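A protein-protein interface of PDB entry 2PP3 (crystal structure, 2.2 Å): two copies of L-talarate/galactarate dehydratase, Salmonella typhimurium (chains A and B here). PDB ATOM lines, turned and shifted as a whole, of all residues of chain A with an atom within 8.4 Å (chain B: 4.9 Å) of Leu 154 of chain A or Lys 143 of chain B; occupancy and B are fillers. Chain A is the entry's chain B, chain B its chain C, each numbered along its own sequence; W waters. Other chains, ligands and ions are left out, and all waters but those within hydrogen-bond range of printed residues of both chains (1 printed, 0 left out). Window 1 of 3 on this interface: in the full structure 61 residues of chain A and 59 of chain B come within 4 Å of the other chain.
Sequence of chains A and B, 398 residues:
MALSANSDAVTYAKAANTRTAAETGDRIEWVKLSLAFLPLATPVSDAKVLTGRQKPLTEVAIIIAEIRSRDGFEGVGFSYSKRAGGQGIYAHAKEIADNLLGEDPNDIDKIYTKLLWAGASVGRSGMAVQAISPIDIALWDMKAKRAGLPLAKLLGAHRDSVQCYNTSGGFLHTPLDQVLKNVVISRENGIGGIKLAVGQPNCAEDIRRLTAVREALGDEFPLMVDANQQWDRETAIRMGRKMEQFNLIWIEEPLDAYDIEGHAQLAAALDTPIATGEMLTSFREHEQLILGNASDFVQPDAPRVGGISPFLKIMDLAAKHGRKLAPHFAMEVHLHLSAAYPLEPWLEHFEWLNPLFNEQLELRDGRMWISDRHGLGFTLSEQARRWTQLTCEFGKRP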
ATOM      1  N   ASN A 106      34.558  19.860 -25.815  1.00  0.00           N
ATOM      2  CA  ASN A 106      33.994  21.148 -26.206  1.00  0.00           C
ATOM      3  C   ASN A 106      34.822  21.895 -27.237  1.00  0.00           C
ATOM      4  O   ASN A 106      34.298  22.750 -27.941  1.00  0.00           O
ATOM      5  CB  ASN A 106      33.786  22.034 -24.981  1.00  0.00           C
ATOM      6  CG  ASN A 106      32.851  21.407 -23.991  1.00  0.00           C
ATOM      7  OD1 ASN A 106      33.264  20.998 -22.908  1.00  0.00           O
ATOM      8  ND2 ASN A 106      31.582  21.288 -24.372  1.00  0.00           N
ATOM      9  N   ILE A 108      35.782  21.610 -30.246  1.00  0.00           N
ATOM     10  CA  ILE A 108      35.498  20.931 -31.492  1.00  0.00           C
ATOM     11  C   ILE A 108      36.463  21.241 -32.641  1.00  0.00           C
ATOM     12  O   ILE A 108      36.930  20.316 -33.308  1.00  0.00           O
ATOM     13  CB  ILE A 108      34.019  21.184 -31.904  1.00  0.00           C
ATOM     14  CG1 ILE A 108      33.092  20.634 -30.805  1.00  0.00           C
ATOM     15  CG2 ILE A 108      33.709  20.494 -33.226  1.00  0.00           C
ATOM     16  CD1 ILE A 108      31.592  20.795 -31.067  1.00  0.00           C
ATOM     17  N   LEU A 139      30.194  15.253 -31.655  1.00  0.00           N
ATOM     18  CA  LEU A 139      30.620  16.249 -30.686  1.00  0.00           C
ATOM     19  C   LEU A 139      29.630  17.418 -30.604  1.00  0.00           C
ATOM     20  O   LEU A 139      29.406  17.963 -29.524  1.00  0.00           O
ATOM     21  CB  LEU A 139      32.022  16.753 -31.025  1.00  0.00           C
ATOM     22  CG  LEU A 139      33.166  15.754 -30.813  1.00  0.00           C
ATOM     23  CD1 LEU A 139      34.490  16.423 -31.169  1.00  0.00           C
ATOM     24  CD2 LEU A 139      33.195  15.291 -29.356  1.00  0.00           C
ATOM     25  N   TRP A 140      29.046  17.810 -31.735  1.00  0.00           N
ATOM     26  CA  TRP A 140      28.065  18.888 -31.720  1.00  0.00           C
ATOM     27  C   TRP A 140      26.798  18.389 -31.015  1.00  0.00           C
ATOM     28  O   TRP A 140      26.141  19.138 -30.283  1.00  0.00           O
ATOM     29  CB  TRP A 140      27.728  19.360 -33.140  1.00  0.00           C
ATOM     30  CG  TRP A 140      28.662  20.423 -33.656  1.00  0.00           C
ATOM     31  CD1 TRP A 140      29.745  20.248 -34.482  1.00  0.00           C
ATOM     32  CD2 TRP A 140      28.619  21.823 -33.344  1.00  0.00           C
ATOM     33  NE1 TRP A 140      30.378  21.457 -34.699  1.00  0.00           N
ATOM     34  CE2 TRP A 140      29.707  22.437 -34.013  1.00  0.00           C
ATOM     35  CE3 TRP A 140      27.766  22.621 -32.562  1.00  0.00           C
ATOM     36  CZ2 TRP A 140      29.962  23.811 -33.923  1.00  0.00           C
ATOM     37  CZ3 TRP A 140      28.020  23.989 -32.474  1.00  0.00           C
ATOM     38  CH2 TRP A 140      29.109  24.571 -33.150  1.00  0.00           C
ATOM     39  N   ASP A 141      26.472  17.118 -31.247  1.00  0.00           N
ATOM     40  CA  ASP A 141      25.309  16.474 -30.633  1.00  0.00           C
ATOM     41  C   ASP A 141      25.514  16.483 -29.118  1.00  0.00           C
ATOM     42  O   ASP A 141      24.588  16.738 -28.353  1.00  0.00           O
ATOM     43  CB  ASP A 141      25.184  15.029 -31.145  1.00  0.00           C
ATOM     44  CG  ASP A 141      24.059  14.247 -30.471  1.00  0.00           C
ATOM     45  OD1 ASP A 141      22.880  14.658 -30.575  1.00  0.00           O
ATOM     46  OD2 ASP A 141      24.359  13.204 -29.844  1.00  0.00           O
ATOM     47  N   MET A 142      26.746  16.226 -28.695  1.00  0.00           N
ATOM     48  CA  MET A 142      27.068  16.199 -27.280  1.00  0.00           C
ATOM     49  C   MET A 142      26.957  17.578 -26.641  1.00  0.00           C
ATOM     50  O   MET A 142      26.358  17.721 -25.570  1.00  0.00           O
ATOM     51  CB  MET A 142      28.479  15.655 -27.053  1.00  0.00           C
ATOM     52  CG  MET A 142      28.843  15.522 -25.575  1.00  0.00           C
ATOM     53  SD  MET A 142      30.559  15.054 -25.278  1.00  0.00           S
ATOM     54  CE  MET A 142      30.480  13.270 -25.633  1.00  0.00           C
ATOM     55  N   LYS A 143      27.532  18.588 -27.291  1.00  0.00           N
ATOM     56  CA  LYS A 143      27.492  19.945 -26.749  1.00  0.00           C
ATOM     57  C   LYS A 143      26.066  20.460 -26.578  1.00  0.00           C
ATOM     58  O   LYS A 143      25.764  21.135 -25.599  1.00  0.00           O
ATOM     59  CB  LYS A 143      28.289  20.909 -27.633  1.00  0.00           C
ATOM     60  CG  LYS A 143      28.278  22.332 -27.125  1.00  0.00           C
ATOM     61  CD  LYS A 143      29.298  23.216 -27.837  1.00  0.00           C
ATOM     62  CE  LYS A 143      30.719  22.826 -27.473  1.00  0.00           C
ATOM     63  NZ  LYS A 143      31.683  23.860 -27.940  1.00  0.00           N
ATOM     64  N   ALA A 144      25.194  20.144 -27.529  1.00  0.00           N
ATOM     65  CA  ALA A 144      23.806  20.578 -27.460  1.00  0.00           C
ATOM     66  C   ALA A 144      23.119  19.910 -26.266  1.00  0.00           C
ATOM     67  O   ALA A 144      22.379  20.557 -25.518  1.00  0.00           O
ATOM     68  CB  ALA A 144      23.078  20.223 -28.755  1.00  0.00           C
ATOM     69  N   LYS A 145      23.366  18.611 -26.098  1.00  0.00           N
ATOM     70  CA  LYS A 145      22.782  17.876 -24.984  1.00  0.00           C
ATOM     71  C   LYS A 145      23.308  18.451 -23.680  1.00  0.00           C
ATOM     72  O   LYS A 145      22.565  18.588 -22.714  1.00  0.00           O
ATOM     73  CB  LYS A 145      23.111  16.381 -25.085  1.00  0.00           C
ATOM     74  CG  LYS A 145      22.302  15.669 -26.149  1.00  0.00           C
ATOM     75  CD  LYS A 145      22.801  14.260 -26.407  1.00  0.00           C
ATOM     76  CE  LYS A 145      21.921  13.567 -27.447  1.00  0.00           C
ATOM     77  NZ  LYS A 145      22.466  12.233 -27.854  1.00  0.00           N
ATOM     78  N   ARG A 146      24.589  18.799 -23.655  1.00  0.00           N
ATOM     79  CA  ARG A 146      25.181  19.380 -22.462  1.00  0.00           C
ATOM     80  C   ARG A 146      24.439  20.669 -22.097  1.00  0.00           C
ATOM     81  O   ARG A 146      24.328  21.022 -20.924  1.00  0.00           O
ATOM     82  CB  ARG A 146      26.654  19.687 -22.701  1.00  0.00           C
ATOM     83  CG  ARG A 146      27.350  20.371 -21.536  1.00  0.00           C
ATOM     84  CD  ARG A 146      28.747  20.805 -21.941  1.00  0.00           C
ATOM     85  NE  ARG A 146      29.552  19.658 -22.341  1.00  0.00           N
ATOM     86  CZ  ARG A 146      30.192  18.862 -21.489  1.00  0.00           C
ATOM     87  NH1 ARG A 146      30.130  19.097 -20.183  1.00  0.00           N
ATOM     88  NH2 ARG A 146      30.890  17.827 -21.945  1.00  0.00           N
ATOM     89  N   ALA A 147      23.932  21.371 -23.107  1.00  0.00           N
ATOM     90  CA  ALA A 147      23.205  22.614 -22.874  1.00  0.00           C
ATOM     91  C   ALA A 147      21.715  22.345 -22.672  1.00  0.00           C
ATOM     92  O   ALA A 147      20.950  23.258 -22.370  1.00  0.00           O
ATOM     93  CB  ALA A 147      23.405  23.564 -24.055  1.00  0.00           C
ATOM     94  N   GLY A 148      21.312  21.089 -22.848  1.00  0.00           N
ATOM     95  CA  GLY A 148      19.916  20.734 -22.692  1.00  0.00           C
ATOM     96  C   GLY A 148      19.071  21.342 -23.795  1.00  0.00           C
ATOM     97  O   GLY A 148      17.961  21.805 -23.553  1.00  0.00           O
ATOM     98  N   LEU A 149      19.585  21.320 -25.023  1.00  0.00           N
ATOM     99  CA  LEU A 149      18.861  21.902 -26.149  1.00  0.00           C
ATOM    100  C   LEU A 149      18.941  21.092 -27.427  1.00  0.00           C
ATOM    101  O   LEU A 149      19.867  20.307 -27.621  1.00  0.00           O
ATOM    102  CB  LEU A 149      19.441  23.272 -26.506  1.00  0.00           C
ATOM    103  CG  LEU A 149      19.623  24.390 -25.495  1.00  0.00           C
ATOM    104  CD1 LEU A 149      20.575  25.426 -26.086  1.00  0.00           C
ATOM    105  CD2 LEU A 149      18.272  25.001 -25.156  1.00  0.00           C
ATOM    106  N   PRO A 150      17.948  21.269 -28.310  1.00  0.00           N
ATOM    107  CA  PRO A 150      17.942  20.570 -29.592  1.00  0.00           C
ATOM    108  C   PRO A 150      19.123  21.268 -30.286  1.00  0.00           C
ATOM    109  O   PRO A 150      19.373  22.449 -30.020  1.00  0.00           O
ATOM    110  CB  PRO A 150      16.607  20.989 -30.206  1.00  0.00           C
ATOM    111  CG  PRO A 150      15.730  21.183 -29.001  1.00  0.00           C
ATOM    112  CD  PRO A 150      16.644  21.906 -28.045  1.00  0.00           C
ATOM    113  N   LEU A 151      19.847  20.578 -31.162  1.00  0.00           N
ATOM    114  CA  LEU A 151      20.999  21.209 -31.814  1.00  0.00           C
ATOM    115  C   LEU A 151      20.694  22.579 -32.408  1.00  0.00           C
ATOM    116  O   LEU A 151      21.476  23.516 -32.250  1.00  0.00           O
ATOM    117  CB  LEU A 151      21.562  20.305 -32.912  1.00  0.00           C
ATOM    118  CG  LEU A 151      22.683  20.912 -33.766  1.00  0.00           C
ATOM    119  CD1 LEU A 151      23.881  21.298 -32.889  1.00  0.00           C
ATOM    120  CD2 LEU A 151      23.111  19.886 -34.824  1.00  0.00           C
ATOM    121  N   ALA A 152      19.560  22.695 -33.087  1.00  0.00           N
ATOM    122  CA  ALA A 152      19.178  23.953 -33.716  1.00  0.00           C
ATOM    123  C   ALA A 152      19.171  25.126 -32.731  1.00  0.00           C
ATOM    124  O   ALA A 152      19.554  26.245 -33.082  1.00  0.00           O
ATOM    125  CB  ALA A 152      17.806  23.805 -34.375  1.00  0.00           C
ATOM    126  N   LYS A 153      18.746  24.869 -31.496  1.00  0.00           N
ATOM    127  CA  LYS A 153      18.698  25.920 -30.486  1.00  0.00           C
ATOM    128  C   LYS A 153      20.092  26.237 -29.983  1.00  0.00           C
ATOM    129  O   LYS A 153      20.376  27.378 -29.635  1.00  0.00           O
ATOM    130  CB  LYS A 153      17.789  25.503 -29.330  1.00  0.00           C
ATOM    131  CG  LYS A 153      16.327  25.413 -29.735  1.00  0.00           C
ATOM    132  CD  LYS A 153      15.759  26.797 -30.017  1.00  0.00           C
ATOM    133  CE  LYS A 153      14.299  26.726 -30.404  1.00  0.00           C
ATOM    134  NZ  LYS A 153      13.719  28.089 -30.563  1.00  0.00           N
ATOM    135  N   LEU A 154      20.969  25.239 -29.939  1.00  0.00           N
ATOM    136  CA  LEU A 154      22.343  25.497 -29.512  1.00  0.00           C
ATOM    137  C   LEU A 154      22.991  26.427 -30.547  1.00  0.00           C
ATOM    138  O   LEU A 154      23.779  27.316 -30.209  1.00  0.00           O
ATOM    139  CB  LEU A 154      23.158  24.203 -29.450  1.00  0.00           C
ATOM    140  CG  LEU A 154      24.662  24.451 -29.249  1.00  0.00           C
ATOM    141  CD1 LEU A 154      24.891  24.925 -27.841  1.00  0.00           C
ATOM    142  CD2 LEU A 154      25.472  23.192 -29.517  1.00  0.00           C
ATOM    143  N   LEU A 155      22.656  26.206 -31.816  1.00  0.00           N
ATOM    144  CA  LEU A 155      23.201  27.016 -32.900  1.00  0.00           C
ATOM    145  C   LEU A 155      22.495  28.365 -32.956  1.00  0.00           C
ATOM    146  O   LEU A 155      23.101  29.379 -33.308  1.00  0.00           O
ATOM    147  CB  LEU A 155      23.021  26.292 -34.238  1.00  0.00           C
ATOM    148  CG  LEU A 155      23.723  24.945 -34.417  1.00  0.00           C
ATOM    149  CD1 LEU A 155      23.304  24.324 -35.743  1.00  0.00           C
ATOM    150  CD2 LEU A 155      25.218  25.141 -34.364  1.00  0.00           C
ATOM    151  N   GLY A 156      21.216  28.366 -32.582  1.00  0.00           N
ATOM    152  CA  GLY A 156      20.419  29.581 -32.623  1.00  0.00           C
ATOM    153  C   GLY A 156      19.560  29.475 -33.865  1.00  0.00           C
ATOM    154  O   GLY A 156      20.061  29.565 -34.979  1.00  0.00           O
ATOM    155  N   ALA A 157      18.265  29.272 -33.679  1.00  0.00           N
ATOM    156  CA  ALA A 157      17.356  29.116 -34.798  1.00  0.00           C
ATOM    157  C   ALA A 157      16.635  30.387 -35.231  1.00  0.00           C
ATOM    158  O   ALA A 157      16.404  31.295 -34.434  1.00  0.00           O
ATOM    159  CB  ALA A 157      16.333  28.035 -34.472  1.00  0.00           C
ATOM    160  N   ILE A 308      29.440  19.301 -39.308  1.00  0.00           N
ATOM    161  CA  ILE A 308      28.737  20.535 -38.994  1.00  0.00           C
ATOM    162  C   ILE A 308      29.659  21.753 -38.982  1.00  0.00           C
ATOM    163  O   ILE A 308      29.297  22.805 -39.506  1.00  0.00           O
ATOM    164  CB  ILE A 308      27.996  20.407 -37.633  1.00  0.00           C
ATOM    165  CG1 ILE A 308      26.780  19.490 -37.806  1.00  0.00           C
ATOM    166  CG2 ILE A 308      27.561  21.781 -37.123  1.00  0.00           C
ATOM    167  CD1 ILE A 308      26.161  19.041 -36.512  1.00  0.00           C
ATOM    168  N   LEU A 312      28.893  24.967 -41.274  1.00  0.00           N
ATOM    169  CA  LEU A 312      28.550  26.272 -40.727  1.00  0.00           C
ATOM    170  C   LEU A 312      29.292  27.382 -41.467  1.00  0.00           C
ATOM    171  O   LEU A 312      28.735  28.455 -41.697  1.00  0.00           O
ATOM    172  CB  LEU A 312      28.868  26.327 -39.226  1.00  0.00           C
ATOM    173  CG  LEU A 312      27.945  25.486 -38.331  1.00  0.00           C
ATOM    174  CD1 LEU A 312      28.461  25.471 -36.915  1.00  0.00           C
ATOM    175  CD2 LEU A 312      26.533  26.042 -38.370  1.00  0.00           C
ATOM    176  N   HIS A 336      18.335  20.784 -38.306  1.00  0.00           N
ATOM    177  CA  HIS A 336      18.919  21.703 -37.334  1.00  0.00           C
ATOM    178  C   HIS A 336      19.759  22.796 -37.983  1.00  0.00           C
ATOM    179  O   HIS A 336      19.729  23.949 -37.548  1.00  0.00           O
ATOM    180  CB  HIS A 336      19.793  20.930 -36.346  1.00  0.00           C
ATOM    181  CG  HIS A 336      19.039  19.938 -35.520  1.00  0.00           C
ATOM    182  ND1 HIS A 336      18.261  20.303 -34.443  1.00  0.00           N
ATOM    183  CD2 HIS A 336      18.909  18.595 -35.640  1.00  0.00           C
ATOM    184  CE1 HIS A 336      17.683  19.229 -33.935  1.00  0.00           C
ATOM    185  NE2 HIS A 336      18.059  18.179 -34.644  1.00  0.00           N
ATOM    186  N   ALA A 340      18.837  27.081 -38.626  1.00  0.00           N
ATOM    187  CA  ALA A 340      19.724  28.173 -38.246  1.00  0.00           C
ATOM    188  C   ALA A 340      20.097  29.087 -39.414  1.00  0.00           C
ATOM    189  O   ALA A 340      20.801  30.071 -39.223  1.00  0.00           O
ATOM    190  CB  ALA A 340      20.997  27.610 -37.605  1.00  0.00           C
ATOM    191  N   GLY A 375      20.151  17.670 -28.594  1.00  0.00           N
ATOM    192  CA  GLY A 375      21.112  17.289 -29.619  1.00  0.00           C
ATOM    193  C   GLY A 375      20.376  17.057 -30.923  1.00  0.00           C
ATOM    194  O   GLY A 375      19.409  17.762 -31.221  1.00  0.00           O
ATOM    195  N   ASN B 106      17.775  31.485 -26.686  1.00  0.00           N
ATOM    196  CA  ASN B 106      18.770  30.738 -27.459  1.00  0.00           C
ATOM    197  C   ASN B 106      18.885  31.163 -28.917  1.00  0.00           C
ATOM    198  O   ASN B 106      19.912  30.926 -29.558  1.00  0.00           O
ATOM    199  CB  ASN B 106      18.482  29.238 -27.392  1.00  0.00           C
ATOM    200  CG  ASN B 106      18.570  28.695 -25.978  1.00  0.00           C
ATOM    201  OD1 ASN B 106      17.562  28.311 -25.393  1.00  0.00           O
ATOM    202  ND2 ASN B 106      19.780  28.671 -25.419  1.00  0.00           N
ATOM    203  N   ILE B 108      19.722  33.714 -30.542  1.00  0.00           N
ATOM    204  CA  ILE B 108      20.440  34.974 -30.480  1.00  0.00           C
ATOM    205  C   ILE B 108      20.400  35.798 -31.762  1.00  0.00           C
ATOM    206  O   ILE B 108      20.104  36.991 -31.723  1.00  0.00           O
ATOM    207  CB  ILE B 108      21.910  34.725 -30.033  1.00  0.00           C
ATOM    208  CG1 ILE B 108      21.903  34.031 -28.659  1.00  0.00           C
ATOM    209  CG2 ILE B 108      22.684  36.044 -29.968  1.00  0.00           C
ATOM    210  CD1 ILE B 108      23.281  33.745 -28.068  1.00  0.00           C
ATOM    211  N   LEU B 139      23.197  37.429 -23.841  1.00  0.00           N
ATOM    212  CA  LEU B 139      22.581  36.195 -24.319  1.00  0.00           C
ATOM    213  C   LEU B 139      23.627  35.080 -24.507  1.00  0.00           C
ATOM    214  O   LEU B 139      23.357  33.914 -24.209  1.00  0.00           O
ATOM    215  CB  LEU B 139      21.818  36.457 -25.622  1.00  0.00           C
ATOM    216  CG  LEU B 139      20.581  37.361 -25.489  1.00  0.00           C
ATOM    217  CD1 LEU B 139      20.071  37.771 -26.861  1.00  0.00           C
ATOM    218  CD2 LEU B 139      19.486  36.623 -24.720  1.00  0.00           C
ATOM    219  N   TRP B 140      24.822  35.431 -24.987  1.00  0.00           N
ATOM    220  CA  TRP B 140      25.875  34.430 -25.164  1.00  0.00           C
ATOM    221  C   TRP B 140      26.328  33.967 -23.783  1.00  0.00           C
ATOM    222  O   TRP B 140      26.581  32.778 -23.562  1.00  0.00           O
ATOM    223  CB  TRP B 140      27.074  34.999 -25.947  1.00  0.00           C
ATOM    224  CG  TRP B 140      26.891  34.970 -27.451  1.00  0.00           C
ATOM    225  CD1 TRP B 140      26.476  35.999 -28.252  1.00  0.00           C
ATOM    226  CD2 TRP B 140      27.077  33.839 -28.316  1.00  0.00           C
ATOM    227  NE1 TRP B 140      26.391  35.577 -29.561  1.00  0.00           N
ATOM    228  CE2 TRP B 140      26.752  34.257 -29.628  1.00  0.00           C
ATOM    229  CE3 TRP B 140      27.483  32.513 -28.111  1.00  0.00           C
ATOM    230  CZ2 TRP B 140      26.820  33.397 -30.728  1.00  0.00           C
ATOM    231  CZ3 TRP B 140      27.551  31.654 -29.209  1.00  0.00           C
ATOM    232  CH2 TRP B 140      27.220  32.101 -30.500  1.00  0.00           C
ATOM    233  N   ASP B 141      26.430  34.919 -22.859  1.00  0.00           N
ATOM    234  CA  ASP B 141      26.814  34.630 -21.479  1.00  0.00           C
ATOM    235  C   ASP B 141      25.791  33.629 -20.929  1.00  0.00           C
ATOM    236  O   ASP B 141      26.147  32.645 -20.281  1.00  0.00           O
ATOM    237  CB  ASP B 141      26.786  35.927 -20.652  1.00  0.00           C
ATOM    238  CG  ASP B 141      27.144  35.712 -19.182  1.00  0.00           C
ATOM    239  OD1 ASP B 141      28.288  35.314 -18.872  1.00  0.00           O
ATOM    240  OD2 ASP B 141      26.269  35.955 -18.326  1.00  0.00           O
ATOM    241  N   MET B 142      24.516  33.866 -21.220  1.00  0.00           N
ATOM    242  CA  MET B 142      23.472  32.970 -20.733  1.00  0.00           C
ATOM    243  C   MET B 142      23.595  31.580 -21.330  1.00  0.00           C
ATOM    244  O   MET B 142      23.510  30.585 -20.615  1.00  0.00           O
ATOM    245  CB  MET B 142      22.083  33.526 -21.048  1.00  0.00           C
ATOM    246  CG  MET B 142      20.948  32.685 -20.475  1.00  0.00           C
ATOM    247  SD  MET B 142      19.297  33.279 -20.949  1.00  0.00           S
ATOM    248  CE  MET B 142      19.105  34.638 -19.754  1.00  0.00           C
ATOM    249  N   LYS B 143      23.791  31.502 -22.643  1.00  0.00           N
ATOM    250  CA  LYS B 143      23.894  30.201 -23.279  1.00  0.00           C
ATOM    251  C   LYS B 143      25.055  29.406 -22.688  1.00  0.00           C
ATOM    252  O   LYS B 143      24.912  28.217 -22.411  1.00  0.00           O
ATOM    253  CB  LYS B 143      24.057  30.342 -24.798  1.00  0.00           C
ATOM    254  CG  LYS B 143      24.032  28.990 -25.527  1.00  0.00           C
ATOM    255  CD  LYS B 143      23.881  29.139 -27.045  1.00  0.00           C
ATOM    256  CE  LYS B 143      22.504  29.666 -27.409  1.00  0.00           C
ATOM    257  NZ  LYS B 143      22.277  29.680 -28.879  1.00  0.00           N
ATOM    258  N   ALA B 144      26.194  30.058 -22.484  1.00  0.00           N
ATOM    259  CA  ALA B 144      27.351  29.371 -21.918  1.00  0.00           C
ATOM    260  C   ALA B 144      26.999  28.812 -20.543  1.00  0.00           C
ATOM    261  O   ALA B 144      27.287  27.654 -20.243  1.00  0.00           O
ATOM    262  CB  ALA B 144      28.546  30.323 -21.815  1.00  0.00           C
ATOM    263  N   LYS B 145      26.366  29.637 -19.711  1.00  0.00           N
ATOM    264  CA  LYS B 145      25.974  29.206 -18.367  1.00  0.00           C
ATOM    265  C   LYS B 145      24.992  28.045 -18.451  1.00  0.00           C
ATOM    266  O   LYS B 145      25.076  27.096 -17.677  1.00  0.00           O
ATOM    267  CB  LYS B 145      25.355  30.378 -17.590  1.00  0.00           C
ATOM    268  CG  LYS B 145      26.382  31.400 -17.154  1.00  0.00           C
ATOM    269  CD  LYS B 145      25.730  32.659 -16.628  1.00  0.00           C
ATOM    270  CE  LYS B 145      26.766  33.640 -16.105  1.00  0.00           C
ATOM    271  NZ  LYS B 145      26.156  34.994 -15.948  1.00  0.00           N
ATOM    272  N   ARG B 146      24.066  28.121 -19.401  1.00  0.00           N
ATOM    273  CA  ARG B 146      23.096  27.052 -19.576  1.00  0.00           C
ATOM    274  C   ARG B 146      23.830  25.731 -19.808  1.00  0.00           C
ATOM    275  O   ARG B 146      23.394  24.676 -19.343  1.00  0.00           O
ATOM    276  CB  ARG B 146      22.193  27.352 -20.774  1.00  0.00           C
ATOM    277  CG  ARG B 146      21.112  26.305 -21.036  1.00  0.00           C
ATOM    278  CD  ARG B 146      20.321  26.657 -22.288  1.00  0.00           C
ATOM    279  NE  ARG B 146      19.695  27.974 -22.184  1.00  0.00           N
ATOM    280  CZ  ARG B 146      18.560  28.221 -21.533  1.00  0.00           C
ATOM    281  NH1 ARG B 146      17.909  27.237 -20.923  1.00  0.00           N
ATOM    282  NH2 ARG B 146      18.084  29.457 -21.486  1.00  0.00           N
ATOM    283  N   ALA B 147      24.954  25.799 -20.520  1.00  0.00           N
ATOM    284  CA  ALA B 147      25.747  24.611 -20.836  1.00  0.00           C
ATOM    285  C   ALA B 147      26.763  24.281 -19.751  1.00  0.00           C
ATOM    286  O   ALA B 147      27.447  23.260 -19.825  1.00  0.00           O
ATOM    287  CB  ALA B 147      26.470  24.808 -22.179  1.00  0.00           C
ATOM    288  N   LEU B 154      32.154  27.148 -24.848  1.00  0.00           N
ATOM    289  CA  LEU B 154      30.893  27.032 -25.579  1.00  0.00           C
ATOM    290  C   LEU B 154      31.200  27.261 -27.065  1.00  0.00           C
ATOM    291  O   LEU B 154      30.638  26.606 -27.937  1.00  0.00           O
ATOM    292  CB  LEU B 154      29.885  28.089 -25.112  1.00  0.00           C
ATOM    293  CG  LEU B 154      28.627  28.154 -25.988  1.00  0.00           C
ATOM    294  CD1 LEU B 154      27.812  26.899 -25.766  1.00  0.00           C
ATOM    295  CD2 LEU B 154      27.797  29.400 -25.674  1.00  0.00           C
HETATM  296  O   HOH W   1      29.149  21.229 -18.532  1.00  0.00           O
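Of the printed residues of chain B, Arg 146 of chain A touches Ala 147 (3.4 Å). Leu 154 of chain A touches just one residue of chain B: Lys 143. Printed residues of chain B within 4 Å of Gly 156 of chain A: Asn 106 (3.4 Å). Lys 143 of chain B touches just these residues of chain A: Lys 153 (3.1 Å) and Leu 154 (3.1 Å). No residue of chain A comes within 4 Å of Ala 144 of chain B. The nearest residue of chain A that does not touch Lys 143 of chain B is Gly 156 of chain A (4.1 Å).
Of the 12 printed residues of chain B, 5 touch a printed residue of chain A. Hydrophobic or aromatic side chains of chain B within 4 Å of the printed part of chain A: Ala 147. Along chain B the printed residues that touch a printed residue of chain A span positions 106 to 154. Printed residues of chain A that touch a printed residue of chain B: Lys 143, Arg 146, Ala 147, Leu 149, Lys 153, Leu 154 and Gly 156. Among the printed residues, no Asp or Glu carboxylate lies within 4 Å of a Lys or Arg side-chain nitrogen of the other chain.
Lys 143 of chain A touches Leu 154 of chain B, and with the chains exchanged Leu 154 of chain A touches Lys 143 of chain B. Arg 146 of chain A touches Ala 147 of chain B, and with the chains exchanged Ala 147 of chain A touches Arg 146 of chain B. Ala 147 of chain B touches its own counterpart, Ala 147 of chain A. 12 positions are printed for both chains.
Water W1 lies within hydrogen-bond range of the guanidinium group (NH1) of Arg 146 of chain A and the backbone carbonyl oxygen (O) of Ala 147 of chain B.
NE of Arg 146 of chain A lies close to ND2 of Asn 106 of chain A, at 3.3 Å. O of Ala 144 of chain A is in hydrogen-bond range of N of Leu 149 of chain A (2.9 Å). The side-chain amino group of Lys 143 of chain A is in hydrogen-bond range of the backbone carbonyl oxygen of Asn 106 of chain A, at 2.8 Å. The backbone NH of Gly 375 of chain A is in hydrogen-bond range of the backbone carbonyl oxygen of Leu 149 of chain A (2.8 Å). The guanidinium group of Arg 146 of chain B sits close to the side-chain amide nitrogen of Asn 106 of chain B, at 3.3 Å. The backbone carbonyl oxygen of Asn 106 of chain B is in hydrogen-bond range of the side-chain amino group of Lys 143 of chain B.
O of Leu 154 of chain A lies within hydrogen-bond range of NZ of Lys 143 of chain B, at 3.1 Å. The side-chain amino group (NZ) of Lys 143 of chain A sits at hydrogen-bond distance from the backbone carbonyl oxygen (O) of Leu 154 of chain B, at 2.9 Å. NZ of Lys 143 of chain B is in hydrogen-bond range of O of Lys 153 of chain A (3.1 Å).
Arg 146 of chain A touches Ala 147 of chain B (CG to O, 3.4 Å). Ala 147 of chain A touches Arg 146 of chain B. Ala 147 of chain A touches Ala 147 of chain B. Asn 106 of chain B touches Leu 149 of chain A (OD1 to CD2, 3.4 Å). Leu 149 of chain A touches Arg 146 of chain B. Asn 106 of chain B touches Lys 153 of chain A (CB to O, 3.5 Å). Gly 156 of chain A touches Asn 106 of chain B.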
